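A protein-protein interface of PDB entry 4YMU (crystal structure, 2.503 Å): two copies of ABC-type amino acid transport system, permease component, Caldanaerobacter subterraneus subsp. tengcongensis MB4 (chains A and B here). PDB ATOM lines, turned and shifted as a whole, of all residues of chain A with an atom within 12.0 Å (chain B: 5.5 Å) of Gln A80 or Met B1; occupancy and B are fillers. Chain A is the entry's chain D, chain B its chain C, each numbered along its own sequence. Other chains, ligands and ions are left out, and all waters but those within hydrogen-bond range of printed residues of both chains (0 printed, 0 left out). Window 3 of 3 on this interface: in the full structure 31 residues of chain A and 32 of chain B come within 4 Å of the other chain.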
ATOM      1  N   VAL A  69       0.332  -0.416  -7.780  1.00  0.00           N
ATOM      2  CA  VAL A  69       1.679   0.054  -8.064  1.00  0.00           C
ATOM      3  C   VAL A  69       2.619  -0.121  -6.866  1.00  0.00           C
ATOM      4  O   VAL A  69       3.770  -0.502  -7.034  1.00  0.00           O
ATOM      5  CB  VAL A  69       1.674   1.495  -8.616  1.00  0.00           C
ATOM      6  CG1 VAL A  69       3.068   2.075  -8.686  1.00  0.00           C
ATOM      7  CG2 VAL A  69       0.997   1.534  -9.981  1.00  0.00           C
ATOM      8  N   LEU A  71       2.238  -2.452  -4.448  1.00  0.00           N
ATOM      9  CA  LEU A  71       2.409  -3.901  -4.341  1.00  0.00           C
ATOM     10  C   LEU A  71       3.536  -4.364  -5.259  1.00  0.00           C
ATOM     11  O   LEU A  71       4.511  -4.969  -4.812  1.00  0.00           O
ATOM     12  CB  LEU A  71       1.128  -4.630  -4.749  1.00  0.00           C
ATOM     13  CG  LEU A  71       0.687  -5.903  -4.007  1.00  0.00           C
ATOM     14  CD1 LEU A  71       0.267  -6.995  -4.981  1.00  0.00           C
ATOM     15  CD2 LEU A  71       1.716  -6.407  -3.017  1.00  0.00           C
ATOM     16  N   LEU A  72       3.380  -4.075  -6.549  1.00  0.00           N
ATOM     17  CA  LEU A  72       4.343  -4.489  -7.559  1.00  0.00           C
ATOM     18  C   LEU A  72       5.718  -3.868  -7.307  1.00  0.00           C
ATOM     19  O   LEU A  72       6.747  -4.540  -7.451  1.00  0.00           O
ATOM     20  CB  LEU A  72       3.841  -4.092  -8.947  1.00  0.00           C
ATOM     21  CG  LEU A  72       2.443  -4.600  -9.286  1.00  0.00           C
ATOM     22  CD1 LEU A  72       2.094  -4.247 -10.708  1.00  0.00           C
ATOM     23  CD2 LEU A  72       2.331  -6.086  -9.047  1.00  0.00           C
ATOM     24  N   LEU A  73       5.729  -2.602  -6.893  1.00  0.00           N
ATOM     25  CA  LEU A  73       6.979  -1.911  -6.610  1.00  0.00           C
ATOM     26  C   LEU A  73       7.736  -2.689  -5.560  1.00  0.00           C
ATOM     27  O   LEU A  73       8.938  -2.892  -5.698  1.00  0.00           O
ATOM     28  CB  LEU A  73       6.748  -0.479  -6.132  1.00  0.00           C
ATOM     29  CG  LEU A  73       8.033   0.302  -5.837  1.00  0.00           C
ATOM     30  CD1 LEU A  73       8.764   0.570  -7.123  1.00  0.00           C
ATOM     31  CD2 LEU A  73       7.760   1.611  -5.106  1.00  0.00           C
ATOM     32  N   ILE A  74       7.039  -3.168  -4.534  1.00  0.00           N
ATOM     33  CA  ILE A  74       7.730  -3.978  -3.549  1.00  0.00           C
ATOM     34  C   ILE A  74       8.117  -5.352  -4.128  1.00  0.00           C
ATOM     35  O   ILE A  74       9.254  -5.809  -3.959  1.00  0.00           O
ATOM     36  CB  ILE A  74       6.927  -4.177  -2.263  1.00  0.00           C
ATOM     37  CG1 ILE A  74       6.660  -2.833  -1.569  1.00  0.00           C
ATOM     38  CG2 ILE A  74       7.682  -5.125  -1.324  1.00  0.00           C
ATOM     39  CD1 ILE A  74       5.913  -2.973  -0.264  1.00  0.00           C
ATOM     40  N   TYR A  75       7.175  -6.007  -4.802  1.00  0.00           N
ATOM     41  CA  TYR A  75       7.376  -7.383  -5.253  1.00  0.00           C
ATOM     42  C   TYR A  75       8.330  -7.499  -6.452  1.00  0.00           C
ATOM     43  O   TYR A  75       9.411  -8.054  -6.337  1.00  0.00           O
ATOM     44  CB  TYR A  75       6.032  -8.045  -5.562  1.00  0.00           C
ATOM     45  CG  TYR A  75       6.119  -9.537  -5.778  1.00  0.00           C
ATOM     46  CD1 TYR A  75       5.915 -10.094  -7.038  1.00  0.00           C
ATOM     47  CD2 TYR A  75       6.395 -10.398  -4.717  1.00  0.00           C
ATOM     48  CE1 TYR A  75       5.982 -11.478  -7.238  1.00  0.00           C
ATOM     49  CE2 TYR A  75       6.477 -11.781  -4.908  1.00  0.00           C
ATOM     50  CZ  TYR A  75       6.268 -12.309  -6.172  1.00  0.00           C
ATOM     51  OH  TYR A  75       6.339 -13.667  -6.370  1.00  0.00           O
ATOM     52  N   ASN A  76       7.918  -6.975  -7.596  1.00  0.00           N
ATOM     53  CA  ASN A  76       8.748  -6.995  -8.787  1.00  0.00           C
ATOM     54  C   ASN A  76       9.935  -6.041  -8.688  1.00  0.00           C
ATOM     55  O   ASN A  76      11.065  -6.401  -9.006  1.00  0.00           O
ATOM     56  CB  ASN A  76       7.907  -6.629 -10.003  1.00  0.00           C
ATOM     57  CG  ASN A  76       6.830  -7.655 -10.288  1.00  0.00           C
ATOM     58  OD1 ASN A  76       6.844  -8.748  -9.712  1.00  0.00           O
ATOM     59  ND2 ASN A  76       5.891  -7.318 -11.181  1.00  0.00           N
ATOM     60  N   GLY A  77       9.686  -4.825  -8.224  1.00  0.00           N
ATOM     61  CA  GLY A  77      10.703  -3.795  -8.241  1.00  0.00           C
ATOM     62  C   GLY A  77      11.908  -4.084  -7.372  1.00  0.00           C
ATOM     63  O   GLY A  77      12.971  -3.497  -7.566  1.00  0.00           O
ATOM     64  N   LEU A  78      11.773  -4.995  -6.420  1.00  0.00           N
ATOM     65  CA  LEU A  78      12.905  -5.266  -5.541  1.00  0.00           C
ATOM     66  C   LEU A  78      13.807  -6.424  -6.013  1.00  0.00           C
ATOM     67  O   LEU A  78      14.939  -6.572  -5.537  1.00  0.00           O
ATOM     68  CB  LEU A  78      12.431  -5.480  -4.104  1.00  0.00           C
ATOM     69  CG  LEU A  78      11.951  -4.193  -3.428  1.00  0.00           C
ATOM     70  CD1 LEU A  78      11.739  -4.415  -1.935  1.00  0.00           C
ATOM     71  CD2 LEU A  78      12.920  -3.044  -3.689  1.00  0.00           C
ATOM     72  N   MET A  79      13.305  -7.224  -6.951  1.00  0.00           N
ATOM     73  CA  MET A  79      14.031  -8.392  -7.451  1.00  0.00           C
ATOM     74  C   MET A  79      15.446  -8.061  -7.943  1.00  0.00           C
ATOM     75  O   MET A  79      16.423  -8.713  -7.548  1.00  0.00           O
ATOM     76  CB  MET A  79      13.214  -9.095  -8.533  1.00  0.00           C
ATOM     77  CG  MET A  79      12.163 -10.040  -7.970  1.00  0.00           C
ATOM     78  SD  MET A  79      10.858 -10.395  -9.167  1.00  0.00           S
ATOM     79  CE  MET A  79       9.771 -11.426  -8.182  1.00  0.00           C
ATOM     80  N   GLN A  80      15.554  -7.028  -8.774  1.00  0.00           N
ATOM     81  CA  GLN A  80      16.836  -6.624  -9.344  1.00  0.00           C
ATOM     82  C   GLN A  80      17.878  -6.218  -8.306  1.00  0.00           C
ATOM     83  O   GLN A  80      19.012  -5.916  -8.656  1.00  0.00           O
ATOM     84  CB  GLN A  80      16.638  -5.487 -10.342  1.00  0.00           C
ATOM     85  CG  GLN A  80      16.083  -4.228  -9.712  1.00  0.00           C
ATOM     86  CD  GLN A  80      15.651  -3.212 -10.741  1.00  0.00           C
ATOM     87  OE1 GLN A  80      14.565  -3.321 -11.338  1.00  0.00           O
ATOM     88  NE2 GLN A  80      16.501  -2.208 -10.960  1.00  0.00           N
ATOM     89  N   PHE A  81      17.492  -6.185  -7.036  1.00  0.00           N
ATOM     90  CA  PHE A  81      18.439  -5.909  -5.965  1.00  0.00           C
ATOM     91  C   PHE A  81      18.763  -7.192  -5.229  1.00  0.00           C
ATOM     92  O   PHE A  81      19.234  -7.162  -4.093  1.00  0.00           O
ATOM     93  CB  PHE A  81      17.883  -4.876  -4.989  1.00  0.00           C
ATOM     94  CG  PHE A  81      17.567  -3.561  -5.627  1.00  0.00           C
ATOM     95  CD1 PHE A  81      18.587  -2.701  -6.007  1.00  0.00           C
ATOM     96  CD2 PHE A  81      16.249  -3.176  -5.845  1.00  0.00           C
ATOM     97  CE1 PHE A  81      18.298  -1.475  -6.603  1.00  0.00           C
ATOM     98  CE2 PHE A  81      15.951  -1.956  -6.441  1.00  0.00           C
ATOM     99  CZ  PHE A  81      16.975  -1.104  -6.820  1.00  0.00           C
ATOM    100  N   GLY A  82      18.474  -8.321  -5.867  1.00  0.00           N
ATOM    101  CA  GLY A  82      18.746  -9.616  -5.270  1.00  0.00           C
ATOM    102  C   GLY A  82      17.794  -9.915  -4.134  1.00  0.00           C
ATOM    103  O   GLY A  82      18.175 -10.488  -3.109  1.00  0.00           O
ATOM    104  N   MET A  83      16.540  -9.528  -4.325  1.00  0.00           N
ATOM    105  CA  MET A  83      15.528  -9.696  -3.302  1.00  0.00           C
ATOM    106  C   MET A  83      14.459 -10.645  -3.817  1.00  0.00           C
ATOM    107  O   MET A  83      13.952 -10.481  -4.931  1.00  0.00           O
ATOM    108  CB  MET A  83      14.908  -8.341  -3.008  1.00  0.00           C
ATOM    109  CG  MET A  83      15.930  -7.282  -2.636  1.00  0.00           C
ATOM    110  SD  MET A  83      16.167  -7.124  -0.858  1.00  0.00           S
ATOM    111  CE  MET A  83      14.524  -6.597  -0.368  1.00  0.00           C
ATOM    112  N   ASN A  84      14.106 -11.629  -3.001  1.00  0.00           N
ATOM    113  CA  ASN A  84      13.065 -12.572  -3.376  1.00  0.00           C
ATOM    114  C   ASN A  84      12.113 -12.771  -2.218  1.00  0.00           C
ATOM    115  O   ASN A  84      11.987 -13.873  -1.681  1.00  0.00           O
ATOM    116  CB  ASN A  84      13.663 -13.906  -3.823  1.00  0.00           C
ATOM    117  CG  ASN A  84      14.181 -13.860  -5.251  1.00  0.00           C
ATOM    118  OD1 ASN A  84      13.467 -13.444  -6.170  1.00  0.00           O
ATOM    119  ND2 ASN A  84      15.426 -14.291  -5.447  1.00  0.00           N
ATOM    120  N   ILE A  85      11.441 -11.681  -1.850  1.00  0.00           N
ATOM    121  CA  ILE A  85      10.489 -11.672  -0.753  1.00  0.00           C
ATOM    122  C   ILE A  85       9.226 -12.409  -1.159  1.00  0.00           C
ATOM    123  O   ILE A  85       8.668 -12.149  -2.235  1.00  0.00           O
ATOM    124  CB  ILE A  85      10.143 -10.221  -0.347  1.00  0.00           C
ATOM    125  CG1 ILE A  85      10.480  -9.262  -1.496  1.00  0.00           C
ATOM    126  CG2 ILE A  85      10.922  -9.821   0.896  1.00  0.00           C
ATOM    127  CD1 ILE A  85      10.247  -7.800  -1.179  1.00  0.00           C
ATOM    128  N   MET B   1      20.480  -4.771 -11.584  1.00  0.00           N
ATOM    129  CA  MET B   1      21.852  -4.343 -11.334  1.00  0.00           C
ATOM    130  C   MET B   1      21.898  -3.336 -10.180  1.00  0.00           C
ATOM    131  O   MET B   1      21.730  -3.694  -9.009  1.00  0.00           O
ATOM    132  CB  MET B   1      22.421  -3.718 -12.608  1.00  0.00           C
ATOM    133  CG  MET B   1      23.937  -3.696 -12.673  1.00  0.00           C
ATOM    134  SD  MET B   1      24.513  -2.569 -13.959  1.00  0.00           S
ATOM    135  CE  MET B   1      23.410  -2.985 -15.305  1.00  0.00           C
ATOM    136  N   THR B   2      22.138  -2.075 -10.524  1.00  0.00           N
ATOM    137  CA  THR B   2      21.916  -0.952  -9.615  1.00  0.00           C
ATOM    138  C   THR B   2      21.032   0.032 -10.382  1.00  0.00           C
ATOM    139  O   THR B   2      20.897  -0.079 -11.603  1.00  0.00           O
ATOM    140  CB  THR B   2      23.217  -0.266  -9.160  1.00  0.00           C
ATOM    141  OG1 THR B   2      24.149  -0.219 -10.245  1.00  0.00           O
ATOM    142  CG2 THR B   2      23.835  -1.014  -7.992  1.00  0.00           C
ATOM    143  N   VAL B   3      20.418   0.985  -9.688  1.00  0.00           N
ATOM    144  CA  VAL B   3      19.389   1.801 -10.333  1.00  0.00           C
ATOM    145  C   VAL B   3      19.958   2.679 -11.459  1.00  0.00           C
ATOM    146  O   VAL B   3      21.070   3.202 -11.354  1.00  0.00           O
ATOM    147  CB  VAL B   3      18.543   2.613  -9.300  1.00  0.00           C
ATOM    148  CG1 VAL B   3      19.189   2.576  -7.912  1.00  0.00           C
ATOM    149  CG2 VAL B   3      18.311   4.038  -9.774  1.00  0.00           C
ATOM    150  N   TYR B 183      15.042  -5.731 -17.933  1.00  0.00           N
ATOM    151  CA  TYR B 183      15.189  -6.504 -16.694  1.00  0.00           C
ATOM    152  C   TYR B 183      15.065  -5.625 -15.434  1.00  0.00           C
ATOM    153  O   TYR B 183      15.380  -6.056 -14.325  1.00  0.00           O
ATOM    154  CB  TYR B 183      16.481  -7.337 -16.698  1.00  0.00           C
ATOM    155  CG  TYR B 183      16.612  -8.139 -17.976  1.00  0.00           C
ATOM    156  CD1 TYR B 183      16.012  -9.388 -18.106  1.00  0.00           C
ATOM    157  CD2 TYR B 183      17.314  -7.629 -19.063  1.00  0.00           C
ATOM    158  CE1 TYR B 183      16.111 -10.103 -19.285  1.00  0.00           C
ATOM    159  CE2 TYR B 183      17.420  -8.335 -20.241  1.00  0.00           C
ATOM    160  CZ  TYR B 183      16.822  -9.572 -20.351  1.00  0.00           C
ATOM    161  OH  TYR B 183      16.940 -10.268 -21.533  1.00  0.00           O
ATOM    162  N   ARG B 184      14.570  -4.401 -15.615  1.00  0.00           N
ATOM    163  CA  ARG B 184      14.385  -3.471 -14.504  1.00  0.00           C
ATOM    164  C   ARG B 184      12.901  -3.268 -14.194  1.00  0.00           C
ATOM    165  O   ARG B 184      12.133  -2.837 -15.054  1.00  0.00           O
ATOM    166  CB  ARG B 184      15.034  -2.125 -14.821  1.00  0.00           C
ATOM    167  CG  ARG B 184      16.538  -2.192 -14.932  1.00  0.00           C
ATOM    168  CD  ARG B 184      17.147  -0.834 -15.214  1.00  0.00           C
ATOM    169  NE  ARG B 184      18.604  -0.879 -15.139  1.00  0.00           N
ATOM    170  CZ  ARG B 184      19.301  -0.923 -14.008  1.00  0.00           C
ATOM    171  NH1 ARG B 184      18.684  -0.913 -12.833  1.00  0.00           N
ATOM    172  NH2 ARG B 184      20.623  -0.968 -14.054  1.00  0.00           N
ATOM    173  N   TYR B 185      12.503  -3.580 -12.965  1.00  0.00           N
ATOM    174  CA  TYR B 185      11.123  -3.356 -12.543  1.00  0.00           C
ATOM    175  C   TYR B 185      10.995  -2.074 -11.718  1.00  0.00           C
ATOM    176  O   TYR B 185      10.108  -1.272 -11.958  1.00  0.00           O
ATOM    177  CB  TYR B 185      10.589  -4.554 -11.751  1.00  0.00           C
ATOM    178  CG  TYR B 185       9.816  -5.563 -12.574  1.00  0.00           C
ATOM    179  CD1 TYR B 185       8.715  -5.174 -13.309  1.00  0.00           C
ATOM    180  CD2 TYR B 185      10.172  -6.909 -12.591  1.00  0.00           C
ATOM    181  CE1 TYR B 185       7.986  -6.085 -14.046  1.00  0.00           C
ATOM    182  CE2 TYR B 185       9.454  -7.832 -13.330  1.00  0.00           C
ATOM    183  CZ  TYR B 185       8.356  -7.416 -14.055  1.00  0.00           C
ATOM    184  OH  TYR B 185       7.611  -8.310 -14.808  1.00  0.00           O
ATOM    185  N   PHE B 186      11.899  -1.900 -10.761  1.00  0.00           N
ATOM    186  CA  PHE B 186      11.931  -0.751  -9.859  1.00  0.00           C
ATOM    187  C   PHE B 186      11.715   0.592 -10.549  1.00  0.00           C
ATOM    188  O   PHE B 186      10.728   1.273 -10.296  1.00  0.00           O
ATOM    189  CB  PHE B 186      13.280  -0.719  -9.159  1.00  0.00           C
ATOM    190  CG  PHE B 186      13.417   0.370  -8.144  1.00  0.00           C
ATOM    191  CD1 PHE B 186      13.157   0.121  -6.810  1.00  0.00           C
ATOM    192  CD2 PHE B 186      13.861   1.634  -8.513  1.00  0.00           C
ATOM    193  CE1 PHE B 186      13.311   1.117  -5.871  1.00  0.00           C
ATOM    194  CE2 PHE B 186      14.008   2.634  -7.575  1.00  0.00           C
ATOM    195  CZ  PHE B 186      13.737   2.376  -6.256  1.00  0.00           C
ATOM    196  N   GLU B 187      12.667   0.985 -11.391  1.00  0.00           N
ATOM    197  CA  GLU B 187      12.652   2.314 -12.014  1.00  0.00           C
ATOM    198  C   GLU B 187      11.388   2.650 -12.824  1.00  0.00           C
ATOM    199  O   GLU B 187      10.850   3.749 -12.694  1.00  0.00           O
ATOM    200  CB  GLU B 187      13.930   2.578 -12.834  1.00  0.00           C
ATOM    201  CG  GLU B 187      14.662   1.334 -13.348  1.00  0.00           C
ATOM    202  CD  GLU B 187      15.662   0.737 -12.369  1.00  0.00           C
ATOM    203  OE1 GLU B 187      15.415  -0.399 -11.917  1.00  0.00           O
ATOM    204  OE2 GLU B 187      16.706   1.366 -12.081  1.00  0.00           O
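N of Met B1 lies within hydrogen-bond range of O of Gln A80.
The side-chain amide nitrogen (NE2) of Gln A80 lies close to the guanidinium group (NH1) of Arg B184 (3.2 Å).
The side-chain amide oxygen of Gln A80 lies within hydrogen-bond range of the backbone NH of Tyr B185, 2.6 Å away.
The backbone NH (N) of Phe B186 sits at hydrogen-bond distance from the side-chain amide oxygen (OE1) of Gln A80.
The side-chain amide oxygen of Gln A80 lies close to the side-chain carboxylate of Glu B187 (3.1 Å).
The guanidinium group (NH2) of Arg B184 is in hydrogen-bond range of the backbone carbonyl oxygen (O) of Thr B2, at 2.6 Å.
NH1 of Arg B184 lies within salt-bridge range of OE2 of Glu B187.
N of Gly A77 lies within hydrogen-bond range of O of Leu A72 (3.1 Å).
Among the printed residues, merely in contact across the chains: Leu A73 with Phe B186, Asn A76 with Tyr B185, Gly A77 with Tyr B185, Gly A77 with Phe B186 and Phe A81 with Phe B186.
Of the printed residues of chain B, Gln A80 touches Met B1 (3.5 Å), Arg B184 (3.2 Å), Tyr B185 (2.6 Å), Phe B186 (3.1 Å) and Glu B187 (2.3 Å).
Of chain A, only Gln A80 (3.5 Å) comes within 4 Å of Met B1.
No residue of chain A comes within 4 Å of Thr B2.
No residue of chain A comes within 4 Å of Val B3.
Arg B184 touches just one residue of chain A: Gln A80 (3.2 Å).
Of the printed residues of chain A, Tyr B185 touches Asn A76 (3.3 Å), Gly A77 (3.6 Å) and Gln A80 (2.6 Å).
Of the printed residues of chain A, Glu B187 touches Gln A80 (2.3 Å).
Met A83 touches none of the printed residues of chain B.
The nearest residue of chain B that does not touch Gln A80 is Tyr B183 (4.1 Å).
The nearest residue of chain A that does not touch Met B1 is Phe A81 (4.5 Å).
The nearest printed residue of chain B that does not touch Phe A81 is Val B3 (4.3 Å).
Hydrophobic or aromatic side chains of chain A that line the printed part of chain B: Leu A73 and Phe A81.
Hydrophobic or aromatic side chains of chain B that line the printed part of chain A: Tyr B185 and Phe B186.
Among the printed residues, 10 pairs touch across the chains.
Among the printed residues, no Asp or Glu carboxylate lies within 4 Å of a Lys or Arg side-chain nitrogen of the other chain.
No position is printed for both chains.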
